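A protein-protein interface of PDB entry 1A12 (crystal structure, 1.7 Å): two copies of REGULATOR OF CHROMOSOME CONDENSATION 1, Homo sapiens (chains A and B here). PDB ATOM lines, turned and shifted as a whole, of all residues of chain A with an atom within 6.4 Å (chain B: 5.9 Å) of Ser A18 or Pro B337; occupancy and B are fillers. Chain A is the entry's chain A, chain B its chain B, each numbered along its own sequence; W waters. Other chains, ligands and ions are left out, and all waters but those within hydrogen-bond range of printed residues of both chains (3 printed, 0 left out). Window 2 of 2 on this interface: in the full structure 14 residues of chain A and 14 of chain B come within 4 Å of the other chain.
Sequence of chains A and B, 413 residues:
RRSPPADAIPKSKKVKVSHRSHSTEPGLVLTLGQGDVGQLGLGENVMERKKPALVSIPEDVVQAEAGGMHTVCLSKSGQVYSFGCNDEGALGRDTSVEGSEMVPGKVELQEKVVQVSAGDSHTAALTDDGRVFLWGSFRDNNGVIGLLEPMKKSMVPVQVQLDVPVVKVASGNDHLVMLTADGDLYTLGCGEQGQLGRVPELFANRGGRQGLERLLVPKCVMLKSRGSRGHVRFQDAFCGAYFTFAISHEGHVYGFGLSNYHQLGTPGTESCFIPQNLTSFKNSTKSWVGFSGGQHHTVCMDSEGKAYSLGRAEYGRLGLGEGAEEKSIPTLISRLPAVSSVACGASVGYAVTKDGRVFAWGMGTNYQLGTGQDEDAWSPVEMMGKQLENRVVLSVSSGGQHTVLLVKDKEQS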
ATOM      1  N   LYS A  16      11.143  -2.845  -0.548  1.00  0.00           N
ATOM      2  CA  LYS A  16      10.442  -3.810   0.316  1.00  0.00           C
ATOM      3  C   LYS A  16      10.449  -3.317   1.763  1.00  0.00           C
ATOM      4  O   LYS A  16      11.367  -2.610   2.195  1.00  0.00           O
ATOM      5  CB  LYS A  16      11.099  -5.190   0.246  1.00  0.00           C
ATOM      6  CG  LYS A  16      11.170  -5.778  -1.147  1.00  0.00           C
ATOM      7  CD  LYS A  16      11.532  -7.250  -1.099  1.00  0.00           C
ATOM      8  CE  LYS A  16      12.058  -7.733  -2.442  1.00  0.00           C
ATOM      9  NZ  LYS A  16      11.169  -7.352  -3.578  1.00  0.00           N
ATOM     10  N   VAL A  17       9.400  -3.685   2.474  1.00  0.00           N
ATOM     11  CA  VAL A  17       9.313  -3.424   3.913  1.00  0.00           C
ATOM     12  C   VAL A  17       9.018  -4.750   4.610  1.00  0.00           C
ATOM     13  O   VAL A  17       8.432  -5.651   4.001  1.00  0.00           O
ATOM     14  CB  VAL A  17       8.066  -2.520   4.242  1.00  0.00           C
ATOM     15  CG1 VAL A  17       8.106  -1.232   3.452  1.00  0.00           C
ATOM     16  CG2 VAL A  17       6.746  -3.269   3.953  1.00  0.00           C
ATOM     17  N   SER A  18       9.347  -4.840   5.885  1.00  0.00           N
ATOM     18  CA  SER A  18       8.976  -6.017   6.666  1.00  0.00           C
ATOM     19  C   SER A  18       8.380  -5.536   7.993  1.00  0.00           C
ATOM     20  O   SER A  18       8.169  -4.331   8.149  1.00  0.00           O
ATOM     21  CB  SER A  18      10.201  -6.906   6.908  1.00  0.00           C
ATOM     22  OG  SER A  18       9.820  -8.178   7.403  1.00  0.00           O
ATOM     23  N   HIS A  19       8.277  -6.429   8.950  1.00  0.00           N
ATOM     24  CA  HIS A  19       7.798  -6.075  10.279  1.00  0.00           C
ATOM     25  C   HIS A  19       8.059  -7.288  11.183  1.00  0.00           C
ATOM     26  O   HIS A  19       8.069  -8.409  10.677  1.00  0.00           O
ATOM     27  CB  HIS A  19       6.306  -5.735  10.267  1.00  0.00           C
ATOM     28  CG  HIS A  19       5.839  -5.044  11.508  1.00  0.00           C
ATOM     29  ND1 HIS A  19       5.053  -5.667  12.458  1.00  0.00           N
ATOM     30  CD2 HIS A  19       6.057  -3.790  11.968  1.00  0.00           C
ATOM     31  CE1 HIS A  19       4.810  -4.821  13.448  1.00  0.00           C
ATOM     32  NE2 HIS A  19       5.409  -3.676  13.173  1.00  0.00           N
ATOM     33  N   ARG A  20       8.168  -7.038  12.478  1.00  0.00           N
ATOM     34  CA  ARG A  20       8.456  -8.150  13.386  1.00  0.00           C
ATOM     35  C   ARG A  20       7.262  -9.091  13.478  1.00  0.00           C
ATOM     36  O   ARG A  20       7.446 -10.223  13.925  1.00  0.00           O
ATOM     37  CB  ARG A  20       8.873  -7.633  14.765  1.00  0.00           C
ATOM     38  CG  ARG A  20       7.907  -6.660  15.409  1.00  0.00           C
ATOM     39  CD  ARG A  20       8.558  -5.995  16.611  1.00  0.00           C
ATOM     40  NE  ARG A  20       7.629  -5.139  17.348  1.00  0.00           N
ATOM     41  CZ  ARG A  20       7.145  -3.984  16.902  1.00  0.00           C
ATOM     42  NH1 ARG A  20       7.493  -3.521  15.707  1.00  0.00           N
ATOM     43  NH2 ARG A  20       6.314  -3.288  17.661  1.00  0.00           N
ATOM     44  N   SER A  21       6.069  -8.632  13.139  1.00  0.00           N
ATOM     45  CA  SER A  21       4.882  -9.473  13.164  1.00  0.00           C
ATOM     46  C   SER A  21       4.773 -10.408  11.985  1.00  0.00           C
ATOM     47  O   SER A  21       3.879 -11.297  12.004  1.00  0.00           O
ATOM     48  CB  SER A  21       3.609  -8.618  13.284  1.00  0.00           C
ATOM     49  OG  SER A  21       3.396  -7.822  12.131  1.00  0.00           O
ATOM     50  N   HIS A  22       5.551 -10.219  10.920  1.00  0.00           N
ATOM     51  CA  HIS A  22       5.346 -11.046   9.707  1.00  0.00           C
ATOM     52  C   HIS A  22       5.857 -12.462   9.939  1.00  0.00           C
ATOM     53  O   HIS A  22       6.956 -12.645  10.491  1.00  0.00           O
ATOM     54  CB  HIS A  22       6.045 -10.415   8.513  1.00  0.00           C
ATOM     55  CG  HIS A  22       5.464  -9.099   8.102  1.00  0.00           C
ATOM     56  ND1 HIS A  22       5.955  -8.369   7.044  1.00  0.00           N
ATOM     57  CD2 HIS A  22       4.428  -8.387   8.606  1.00  0.00           C
ATOM     58  CE1 HIS A  22       5.248  -7.262   6.912  1.00  0.00           C
ATOM     59  NE2 HIS A  22       4.316  -7.248   7.845  1.00  0.00           N
ATOM     60  N   VAL A 114       2.873 -10.722   2.265  1.00  0.00           N
ATOM     61  CA  VAL A 114       3.703 -11.051   3.416  1.00  0.00           C
ATOM     62  C   VAL A 114       2.906 -11.158   4.717  1.00  0.00           C
ATOM     63  O   VAL A 114       3.404 -11.735   5.697  1.00  0.00           O
ATOM     64  CB  VAL A 114       4.839 -10.026   3.616  1.00  0.00           C
ATOM     65  CG1 VAL A 114       5.842 -10.133   2.481  1.00  0.00           C
ATOM     66  CG2 VAL A 114       4.274  -8.612   3.696  1.00  0.00           C
ATOM     67  N   ASP A 128       4.740  -7.176  -0.178  1.00  0.00           N
ATOM     68  CA  ASP A 128       6.108  -6.992   0.291  1.00  0.00           C
ATOM     69  C   ASP A 128       6.607  -5.566   0.230  1.00  0.00           C
ATOM     70  O   ASP A 128       7.642  -5.271   0.898  1.00  0.00           O
ATOM     71  CB  ASP A 128       7.068  -7.952  -0.421  1.00  0.00           C
ATOM     72  CG  ASP A 128       7.069  -7.792  -1.934  1.00  0.00           C
ATOM     73  OD1 ASP A 128       6.214  -7.066  -2.489  1.00  0.00           O
ATOM     74  OD2 ASP A 128       7.941  -8.411  -2.576  1.00  0.00           O
ATOM     75  N   VAL A 166       2.585   0.500   4.528  1.00  0.00           N
ATOM     76  CA  VAL A 166       1.968  -0.148   5.677  1.00  0.00           C
ATOM     77  C   VAL A 166       2.837  -1.325   6.099  1.00  0.00           C
ATOM     78  O   VAL A 166       3.347  -2.047   5.228  1.00  0.00           O
ATOM     79  CB  VAL A 166       0.543  -0.652   5.350  1.00  0.00           C
ATOM     80  CG1 VAL A 166      -0.028  -1.433   6.527  1.00  0.00           C
ATOM     81  CG2 VAL A 166      -0.362   0.521   5.015  1.00  0.00           C
ATOM     82  N   VAL A 167       3.100  -1.448   7.396  1.00  0.00           N
ATOM     83  CA  VAL A 167       3.906  -2.564   7.883  1.00  0.00           C
ATOM     84  C   VAL A 167       3.090  -3.634   8.559  1.00  0.00           C
ATOM     85  O   VAL A 167       3.589  -4.759   8.736  1.00  0.00           O
ATOM     86  CB  VAL A 167       5.029  -2.084   8.834  1.00  0.00           C
ATOM     87  CG1 VAL A 167       6.050  -1.259   8.062  1.00  0.00           C
ATOM     88  CG2 VAL A 167       4.446  -1.269   9.979  1.00  0.00           C
ATOM     89  N   GLY B 305      13.207  -6.944  20.611  1.00  0.00           N
ATOM     90  CA  GLY B 305      13.451  -7.185  19.202  1.00  0.00           C
ATOM     91  C   GLY B 305      13.233  -5.989  18.301  1.00  0.00           C
ATOM     92  O   GLY B 305      13.013  -6.143  17.079  1.00  0.00           O
ATOM     93  N   SER B 334      10.579   0.602  12.003  1.00  0.00           N
ATOM     94  CA  SER B 334       9.503  -0.374  12.015  1.00  0.00           C
ATOM     95  C   SER B 334       9.651  -1.436  10.945  1.00  0.00           C
ATOM     96  O   SER B 334       9.064  -2.531  11.054  1.00  0.00           O
ATOM     97  CB  SER B 334       8.155   0.329  11.853  1.00  0.00           C
ATOM     98  OG  SER B 334       8.079   0.997  10.606  1.00  0.00           O
ATOM     99  N   ARG B 335      10.353  -1.124   9.865  1.00  0.00           N
ATOM    100  CA  ARG B 335      10.433  -1.983   8.694  1.00  0.00           C
ATOM    101  C   ARG B 335      11.269  -3.225   8.864  1.00  0.00           C
ATOM    102  O   ARG B 335      11.345  -4.027   7.890  1.00  0.00           O
ATOM    103  CB  ARG B 335      10.978  -1.186   7.503  1.00  0.00           C
ATOM    104  CG  ARG B 335      10.111  -0.026   7.035  1.00  0.00           C
ATOM    105  CD  ARG B 335      10.838   0.766   5.956  1.00  0.00           C
ATOM    106  NE  ARG B 335       9.986   1.744   5.284  1.00  0.00           N
ATOM    107  CZ  ARG B 335       9.717   2.961   5.747  1.00  0.00           C
ATOM    108  NH1 ARG B 335      10.228   3.374   6.899  1.00  0.00           N
ATOM    109  NH2 ARG B 335       8.940   3.777   5.046  1.00  0.00           N
ATOM    110  N   LEU B 336      11.843  -3.505  10.010  1.00  0.00           N
ATOM    111  CA  LEU B 336      12.683  -4.688  10.201  1.00  0.00           C
ATOM    112  C   LEU B 336      11.915  -5.843  10.828  1.00  0.00           C
ATOM    113  O   LEU B 336      11.090  -5.614  11.719  1.00  0.00           O
ATOM    114  CB  LEU B 336      13.865  -4.339  11.112  1.00  0.00           C
ATOM    115  CG  LEU B 336      14.849  -3.264  10.646  1.00  0.00           C
ATOM    116  CD1 LEU B 336      15.706  -2.808  11.812  1.00  0.00           C
ATOM    117  CD2 LEU B 336      15.705  -3.810   9.522  1.00  0.00           C
ATOM    118  N   PRO B 337      12.302  -7.074  10.519  1.00  0.00           N
ATOM    119  CA  PRO B 337      11.910  -8.236  11.309  1.00  0.00           C
ATOM    120  C   PRO B 337      12.438  -8.092  12.732  1.00  0.00           C
ATOM    121  O   PRO B 337      13.151  -7.143  13.062  1.00  0.00           O
ATOM    122  CB  PRO B 337      12.602  -9.389  10.582  1.00  0.00           C
ATOM    123  CG  PRO B 337      12.648  -8.917   9.166  1.00  0.00           C
ATOM    124  CD  PRO B 337      13.078  -7.486   9.338  1.00  0.00           C
ATOM    125  N   ALA B 338      12.134  -9.061  13.601  1.00  0.00           N
ATOM    126  CA  ALA B 338      12.615  -9.001  14.979  1.00  0.00           C
ATOM    127  C   ALA B 338      14.151  -8.935  14.990  1.00  0.00           C
ATOM    128  O   ALA B 338      14.800  -9.683  14.277  1.00  0.00           O
ATOM    129  CB  ALA B 338      12.131 -10.216  15.756  1.00  0.00           C
ATOM    130  N   VAL B 339      14.697  -8.069  15.830  1.00  0.00           N
ATOM    131  CA  VAL B 339      16.129  -7.772  15.784  1.00  0.00           C
ATOM    132  C   VAL B 339      16.927  -8.418  16.883  1.00  0.00           C
ATOM    133  O   VAL B 339      16.511  -8.414  18.059  1.00  0.00           O
ATOM    134  CB  VAL B 339      16.391  -6.239  15.788  1.00  0.00           C
ATOM    135  CG1 VAL B 339      17.888  -5.943  15.805  1.00  0.00           C
ATOM    136  CG2 VAL B 339      15.753  -5.596  14.566  1.00  0.00           C
ATOM    137  N   THR B 353      18.910  -9.904  12.162  1.00  0.00           N
ATOM    138  CA  THR B 353      17.589 -10.302  12.705  1.00  0.00           C
ATOM    139  C   THR B 353      17.736 -11.581  13.528  1.00  0.00           C
ATOM    140  O   THR B 353      18.651 -12.378  13.312  1.00  0.00           O
ATOM    141  CB  THR B 353      16.598 -10.560  11.562  1.00  0.00           C
ATOM    142  OG1 THR B 353      17.135 -11.560  10.690  1.00  0.00           O
ATOM    143  CG2 THR B 353      16.366  -9.290  10.766  1.00  0.00           C
ATOM    144  N   ASP B 355      16.114 -14.234  13.050  1.00  0.00           N
ATOM    145  CA  ASP B 355      16.166 -15.372  12.121  1.00  0.00           C
ATOM    146  C   ASP B 355      17.401 -15.454  11.241  1.00  0.00           C
ATOM    147  O   ASP B 355      17.447 -16.260  10.309  1.00  0.00           O
ATOM    148  CB  ASP B 355      14.915 -15.471  11.217  1.00  0.00           C
ATOM    149  CG  ASP B 355      14.751 -14.282  10.273  1.00  0.00           C
ATOM    150  OD1 ASP B 355      15.730 -13.562   9.995  1.00  0.00           O
ATOM    151  OD2 ASP B 355      13.603 -14.042   9.845  1.00  0.00           O
ATOM    152  N   ARG B 357      19.142 -12.980   9.318  1.00  0.00           N
ATOM    153  CA  ARG B 357      19.344 -12.152   8.118  1.00  0.00           C
ATOM    154  C   ARG B 357      20.023 -10.842   8.500  1.00  0.00           C
ATOM    155  O   ARG B 357      20.009 -10.465   9.671  1.00  0.00           O
ATOM    156  CB  ARG B 357      18.004 -11.890   7.428  1.00  0.00           C
ATOM    157  CG  ARG B 357      17.373 -13.146   6.840  1.00  0.00           C
ATOM    158  CD  ARG B 357      16.007 -12.870   6.234  1.00  0.00           C
ATOM    159  NE  ARG B 357      14.977 -12.664   7.244  1.00  0.00           N
ATOM    160  CZ  ARG B 357      13.822 -12.047   7.021  1.00  0.00           C
ATOM    161  NH1 ARG B 357      13.542 -11.563   5.821  1.00  0.00           N
ATOM    162  NH2 ARG B 357      12.934 -11.925   8.001  1.00  0.00           N
ATOM    163  N   PHE B 359      20.157  -6.598   7.430  1.00  0.00           N
ATOM    164  CA  PHE B 359      19.582  -5.474   6.701  1.00  0.00           C
ATOM    165  C   PHE B 359      20.533  -4.272   6.818  1.00  0.00           C
ATOM    166  O   PHE B 359      21.205  -4.124   7.833  1.00  0.00           O
ATOM    167  CB  PHE B 359      18.203  -5.119   7.257  1.00  0.00           C
ATOM    168  CG  PHE B 359      17.137  -6.123   6.920  1.00  0.00           C
ATOM    169  CD1 PHE B 359      17.166  -7.403   7.469  1.00  0.00           C
ATOM    170  CD2 PHE B 359      16.104  -5.792   6.050  1.00  0.00           C
ATOM    171  CE1 PHE B 359      16.180  -8.338   7.155  1.00  0.00           C
ATOM    172  CE2 PHE B 359      15.114  -6.719   5.730  1.00  0.00           C
ATOM    173  CZ  PHE B 359      15.153  -7.994   6.283  1.00  0.00           C
HETATM  174  O   HOH W   1      11.139 -10.083   5.426  1.00  0.00           O
HETATM  175  O   HOH W   2      10.231 -11.023   7.964  1.00  0.00           O
HETATM  176  O   HOH W   3       9.254  -4.221  13.298  1.00  0.00           O
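The backbone carbonyl oxygen (O) of Asp A128 sits at hydrogen-bond distance from the backbone NH (N) of Val A17 (2.8 Å). A ring nitrogen (NE2) of His A19 is in hydrogen-bond range of the guanidinium group (NH1) of Arg A20. A ring nitrogen (ND1) of His A19 lies within hydrogen-bond range of the side-chain hydroxyl of Ser A21, 2.7 Å away. The backbone carbonyl oxygen of Val A167 is in hydrogen-bond range of a ring nitrogen (NE2) of His A22, at 2.7 Å.
The backbone NH (N) of Ser A18 lies within hydrogen-bond range of the backbone carbonyl oxygen (O) of Arg B335, 2.9 Å away. The backbone carbonyl oxygen (O) of Leu B336 is in hydrogen-bond range of the backbone NH (N) of Arg A20.
Ser A18 touches three residues of chain B. Printed residues of chain A within 4 Å of Pro B337: Ser A18 and His A19. Printed residues of chain A within 4 Å of Leu B336: His A19 (3.5 Å) and Arg A20 (3.3 Å). Of the printed residues of chain A, Ser B334 touches Ser A18, His A19 and Val A167. Val B339 touches none of the printed residues of chain A. Val A166 touches none of the printed residues of chain B. The nearest residue of chain B that does not touch Ser A18 is Leu B336 (4.2 Å). The nearest residue of chain A that does not touch Pro B337 is Arg A20 (4.03 Å).
Hydrophobic or aromatic side chains of chain A within 4 Å of the printed part of chain B: Val A17, His A19 and Val A167. Printed residues of chain B that touch a printed residue of chain A: Ser B334, Arg B335, Leu B336, Pro B337 and Ala B338. Among the printed residues, 10 pairs touch across the chains.
Arg B335 touches Val A17. Ser A18 touches Ser B334. Ser A18 touches Pro B337 (OG to CG, 3.4 Å). His A19 touches Ser B334. C of His A19 touches O of Leu B336, 3.5 Å away. O of His A19 touches CA of Pro B337, at 3.9 Å. CB of Arg A20 touches N of Ala B338, 3.7 Å away. Val A167 touches Ser B334 (CG1 to OG, 3.96 Å).
Water W3 lies within hydrogen-bond range of O of Leu B336 (2.8 Å), O of Ser B334 (2.8 Å) and NH1 of Arg A20 (3.1 Å). Water W2 bridges the guanidinium group (NH2) of Arg B357 and the side-chain hydroxyl (OG) of Ser A18. Water W1 bridges the guanidinium group of Arg B357 (2.8 Å) and the side-chain hydroxyl of Ser A18 (3.0 Å).
No position is printed for both chains. Of the 10 pairs that touch across the chains among the printed residues, none has its exchanged pair printed and touching as well.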
